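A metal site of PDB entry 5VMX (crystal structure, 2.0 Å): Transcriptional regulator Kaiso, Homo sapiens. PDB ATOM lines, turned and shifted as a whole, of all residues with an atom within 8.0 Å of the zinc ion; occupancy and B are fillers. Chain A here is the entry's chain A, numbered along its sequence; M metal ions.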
ATOM      1  N   PRO A  53       0.750  25.348  10.834  1.00  0.00           N
ATOM      2  CA  PRO A  53      -0.057  25.818  11.972  1.00  0.00           C
ATOM      3  C   PRO A  53      -0.848  24.685  12.641  1.00  0.00           C
ATOM      4  O   PRO A  53      -1.378  23.830  11.927  1.00  0.00           O
ATOM      5  CB  PRO A  53      -1.005  26.818  11.322  1.00  0.00           C
ATOM      6  CG  PRO A  53      -1.198  26.307   9.928  1.00  0.00           C
ATOM      7  CD  PRO A  53       0.097  25.604   9.538  1.00  0.00           C
ATOM      8  N   CYS A  54      -0.900  24.681  13.985  1.00  0.00           N
ATOM      9  CA  CYS A  54      -1.678  23.694  14.751  1.00  0.00           C
ATOM     10  C   CYS A  54      -3.150  23.894  14.427  1.00  0.00           C
ATOM     11  O   CYS A  54      -3.608  25.034  14.345  1.00  0.00           O
ATOM     12  CB  CYS A  54      -1.431  23.842  16.271  1.00  0.00           C
ATOM     13  SG  CYS A  54      -2.514  22.840  17.427  1.00  0.00           S
ATOM     14  N   ARG A  55      -3.880  22.831  14.181  1.00  0.00           N
ATOM     15  CA  ARG A  55      -5.283  22.925  13.899  1.00  0.00           C
ATOM     16  C   ARG A  55      -6.171  23.126  15.118  1.00  0.00           C
ATOM     17  O   ARG A  55      -7.353  23.178  14.974  1.00  0.00           O
ATOM     18  CB  ARG A  55      -5.734  21.705  13.138  1.00  0.00           C
ATOM     19  CG  ARG A  55      -5.455  21.776  11.654  1.00  0.00           C
ATOM     20  CD  ARG A  55      -3.977  21.894  11.360  1.00  0.00           C
ATOM     21  NE  ARG A  55      -3.276  20.631  11.543  1.00  0.00           N
ATOM     22  CZ  ARG A  55      -2.953  19.797  10.574  1.00  0.00           C
ATOM     23  NH1 ARG A  55      -3.249  20.095   9.332  1.00  0.00           N
ATOM     24  NH2 ARG A  55      -2.333  18.683  10.847  1.00  0.00           N
ATOM     25  N   TYR A  56      -5.603  23.177  16.307  1.00  0.00           N
ATOM     26  CA  TYR A  56      -6.397  23.259  17.547  1.00  0.00           C
ATOM     27  C   TYR A  56      -6.081  24.489  18.355  1.00  0.00           C
ATOM     28  O   TYR A  56      -6.873  24.892  19.218  1.00  0.00           O
ATOM     29  CB  TYR A  56      -6.178  22.024  18.431  1.00  0.00           C
ATOM     30  CG  TYR A  56      -6.445  20.715  17.748  1.00  0.00           C
ATOM     31  CD1 TYR A  56      -7.719  20.161  17.749  1.00  0.00           C
ATOM     32  CD2 TYR A  56      -5.433  20.029  17.105  1.00  0.00           C
ATOM     33  CE1 TYR A  56      -7.963  18.947  17.121  1.00  0.00           C
ATOM     34  CE2 TYR A  56      -5.668  18.826  16.481  1.00  0.00           C
ATOM     35  CZ  TYR A  56      -6.938  18.282  16.498  1.00  0.00           C
ATOM     36  OH  TYR A  56      -7.152  17.083  15.866  1.00  0.00           O
ATOM     37  N   CYS A  57      -4.921  25.080  18.113  1.00  0.00           N
ATOM     38  CA  CYS A  57      -4.573  26.336  18.752  1.00  0.00           C
ATOM     39  C   CYS A  57      -3.818  27.217  17.757  1.00  0.00           C
ATOM     40  O   CYS A  57      -3.752  26.919  16.569  1.00  0.00           O
ATOM     41  CB  CYS A  57      -3.746  26.111  20.039  1.00  0.00           C
ATOM     42  SG  CYS A  57      -1.995  25.692  19.841  1.00  0.00           S
ATOM     43  N   GLU A  58      -3.260  28.321  18.255  1.00  0.00           N
ATOM     44  CA  GLU A  58      -2.682  29.340  17.390  1.00  0.00           C
ATOM     45  C   GLU A  58      -1.204  29.089  17.057  1.00  0.00           C
ATOM     46  O   GLU A  58      -0.616  29.814  16.270  1.00  0.00           O
ATOM     47  CB  GLU A  58      -2.845  30.722  18.044  1.00  0.00           C
ATOM     48  CG  GLU A  58      -2.005  30.961  19.307  1.00  0.00           C
ATOM     49  CD  GLU A  58      -2.345  30.015  20.462  1.00  0.00           C
ATOM     50  OE1 GLU A  58      -1.416  29.684  21.227  1.00  0.00           O
ATOM     51  OE2 GLU A  58      -3.525  29.620  20.605  1.00  0.00           O
ATOM     52  N   LYS A  59      -0.616  28.035  17.636  1.00  0.00           N
ATOM     53  CA  LYS A  59       0.823  27.793  17.462  1.00  0.00           C
ATOM     54  C   LYS A  59       1.186  27.367  16.039  1.00  0.00           C
ATOM     55  O   LYS A  59       0.425  26.688  15.358  1.00  0.00           O
ATOM     56  CB  LYS A  59       1.304  26.734  18.455  1.00  0.00           C
ATOM     57  CG  LYS A  59       1.287  27.221  19.897  1.00  0.00           C
ATOM     58  CD  LYS A  59       2.013  26.242  20.810  1.00  0.00           C
ATOM     59  CE  LYS A  59       3.498  26.277  20.556  1.00  0.00           C
ATOM     60  NZ  LYS A  59       4.208  25.261  21.387  1.00  0.00           N
ATOM     61  N   VAL A  60       2.377  27.783  15.590  1.00  0.00           N
ATOM     62  CA  VAL A  60       2.840  27.467  14.245  1.00  0.00           C
ATOM     63  C   VAL A  60       4.274  26.922  14.280  1.00  0.00           C
ATOM     64  O   VAL A  60       5.116  27.435  15.015  1.00  0.00           O
ATOM     65  CB  VAL A  60       2.776  28.707  13.337  1.00  0.00           C
ATOM     66  CG1 VAL A  60       3.212  28.350  11.928  1.00  0.00           C
ATOM     67  CG2 VAL A  60       1.372  29.295  13.329  1.00  0.00           C
ATOM     68  N   PHE A  61       4.535  25.879  13.483  1.00  0.00           N
ATOM     69  CA  PHE A  61       5.811  25.162  13.517  1.00  0.00           C
ATOM     70  C   PHE A  61       6.541  25.199  12.177  1.00  0.00           C
ATOM     71  O   PHE A  61       5.890  25.254  11.131  1.00  0.00           O
ATOM     72  CB  PHE A  61       5.572  23.700  13.944  1.00  0.00           C
ATOM     73  CG  PHE A  61       4.875  23.573  15.274  1.00  0.00           C
ATOM     74  CD1 PHE A  61       3.505  23.621  15.353  1.00  0.00           C
ATOM     75  CD2 PHE A  61       5.616  23.418  16.438  1.00  0.00           C
ATOM     76  CE1 PHE A  61       2.867  23.516  16.584  1.00  0.00           C
ATOM     77  CE2 PHE A  61       4.990  23.306  17.658  1.00  0.00           C
ATOM     78  CZ  PHE A  61       3.612  23.361  17.735  1.00  0.00           C
ATOM     79  N   ARG A  67       4.651  19.863  14.343  1.00  0.00           N
ATOM     80  CA  ARG A  67       3.223  20.118  14.445  1.00  0.00           C
ATOM     81  C   ARG A  67       2.455  18.829  14.752  1.00  0.00           C
ATOM     82  O   ARG A  67       1.555  18.819  15.603  1.00  0.00           O
ATOM     83  CB  ARG A  67       2.669  20.736  13.173  1.00  0.00           C
ATOM     84  CG  ARG A  67       1.133  20.748  13.226  1.00  0.00           C
ATOM     85  CD  ARG A  67       0.510  21.419  12.079  1.00  0.00           C
ATOM     86  NE  ARG A  67       0.743  20.714  10.840  1.00  0.00           N
ATOM     87  CZ  ARG A  67       0.252  21.108   9.675  1.00  0.00           C
ATOM     88  NH1 ARG A  67      -0.515  22.186   9.625  1.00  0.00           N
ATOM     89  NH2 ARG A  67       0.515  20.429   8.569  1.00  0.00           N
ATOM     90  N   HIS A  70       2.887  17.809  18.257  1.00  0.00           N
ATOM     91  CA  HIS A  70       2.142  18.742  19.094  1.00  0.00           C
ATOM     92  C   HIS A  70       0.631  18.480  19.125  1.00  0.00           C
ATOM     93  O   HIS A  70      -0.012  18.573  20.181  1.00  0.00           O
ATOM     94  CB  HIS A  70       2.396  20.165  18.605  1.00  0.00           C
ATOM     95  CG  HIS A  70       1.484  21.174  19.212  1.00  0.00           C
ATOM     96  ND1 HIS A  70       1.657  21.651  20.500  1.00  0.00           N
ATOM     97  CD2 HIS A  70       0.367  21.789  18.738  1.00  0.00           C
ATOM     98  CE1 HIS A  70       0.710  22.530  20.774  1.00  0.00           C
ATOM     99  NE2 HIS A  70      -0.076  22.633  19.714  1.00  0.00           N
ATOM    100  N   GLU A  71       0.048  18.168  17.975  1.00  0.00           N
ATOM    101  CA  GLU A  71      -1.379  17.932  17.887  1.00  0.00           C
ATOM    102  C   GLU A  71      -1.830  16.668  18.642  1.00  0.00           C
ATOM    103  O   GLU A  71      -2.946  16.611  19.243  1.00  0.00           O
ATOM    104  CB  GLU A  71      -1.791  17.872  16.418  1.00  0.00           C
ATOM    105  CG  GLU A  71      -1.708  19.269  15.764  1.00  0.00           C
ATOM    106  CD  GLU A  71      -2.133  19.267  14.320  1.00  0.00           C
ATOM    107  OE1 GLU A  71      -2.078  18.190  13.686  1.00  0.00           O
ATOM    108  OE2 GLU A  71      -2.542  20.331  13.817  1.00  0.00           O
ATOM    109  N   ILE A  72      -0.953  15.663  18.620  1.00  0.00           N
ATOM    110  CA  ILE A  72      -1.174  14.486  19.464  1.00  0.00           C
ATOM    111  C   ILE A  72      -1.447  14.850  20.943  1.00  0.00           C
ATOM    112  O   ILE A  72      -2.320  14.259  21.583  1.00  0.00           O
ATOM    113  CB  ILE A  72       0.016  13.514  19.366  1.00  0.00           C
ATOM    114  CG1 ILE A  72      -0.179  12.578  18.174  1.00  0.00           C
ATOM    115  CG2 ILE A  72       0.154  12.667  20.621  1.00  0.00           C
ATOM    116  CD1 ILE A  72      -1.240  11.526  18.414  1.00  0.00           C
ATOM    117  N   HIS A  73      -0.726  15.839  21.481  1.00  0.00           N
ATOM    118  CA  HIS A  73      -1.022  16.355  22.832  1.00  0.00           C
ATOM    119  C   HIS A  73      -2.439  16.903  22.985  1.00  0.00           C
ATOM    120  O   HIS A  73      -3.045  16.801  24.062  1.00  0.00           O
ATOM    121  CB  HIS A  73      -0.022  17.459  23.212  1.00  0.00           C
ATOM    122  CG  HIS A  73       1.334  16.947  23.604  1.00  0.00           C
ATOM    123  ND1 HIS A  73       1.751  16.868  24.909  1.00  0.00           N
ATOM    124  CD2 HIS A  73       2.361  16.491  22.847  1.00  0.00           C
ATOM    125  CE1 HIS A  73       2.982  16.381  24.949  1.00  0.00           C
ATOM    126  NE2 HIS A  73       3.367  16.144  23.703  1.00  0.00           N
ATOM    127  N   HIS A  74      -2.964  17.527  21.944  1.00  0.00           N
ATOM    128  CA  HIS A  74      -4.350  17.985  21.979  1.00  0.00           C
ATOM    129  C   HIS A  74      -5.326  16.815  22.047  1.00  0.00           C
ATOM    130  O   HIS A  74      -6.319  16.894  22.764  1.00  0.00           O
ATOM    131  CB  HIS A  74      -4.689  18.843  20.760  1.00  0.00           C
ATOM    132  CG  HIS A  74      -4.160  20.243  20.832  1.00  0.00           C
ATOM    133  ND1 HIS A  74      -4.645  21.175  21.724  1.00  0.00           N
ATOM    134  CD2 HIS A  74      -3.210  20.894  20.101  1.00  0.00           C
ATOM    135  CE1 HIS A  74      -4.027  22.334  21.533  1.00  0.00           C
ATOM    136  NE2 HIS A  74      -3.153  22.189  20.559  1.00  0.00           N
HETATM  137 ZN    ZN M   1      -1.943  23.434  19.437  1.00  0.00          ZN
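Of the 15 residues printed, 4 come within 4 Å of the zinc ion.
The nearest printed residue that does not touch the zinc ion is Tyr 56 (4.4 Å).
The backbone NH (N) of Cys 54 lies within hydrogen-bond range of the backbone carbonyl oxygen (O) of Lys 59.
The backbone NH (N) of Tyr 56 lies close to the side-chain sulfur (SG) of Cys 54, at 3.3 Å.
The backbone NH of Lys 59 sits close to the side-chain sulfur of Cys 57 (3.5 Å).
A ring nitrogen (NE2) of His 70 binds the zinc ion, at 2.1 Å.
NE2 of His 74 is bound to the zinc ion, 2.1 Å away.
SG of Cys 54 binds the zinc ion (2.2 Å).
The side-chain sulfur (SG) of Cys 57 is bound to the zinc ion (2.3 Å).
The zinc ion has four donor atoms within binding distance.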
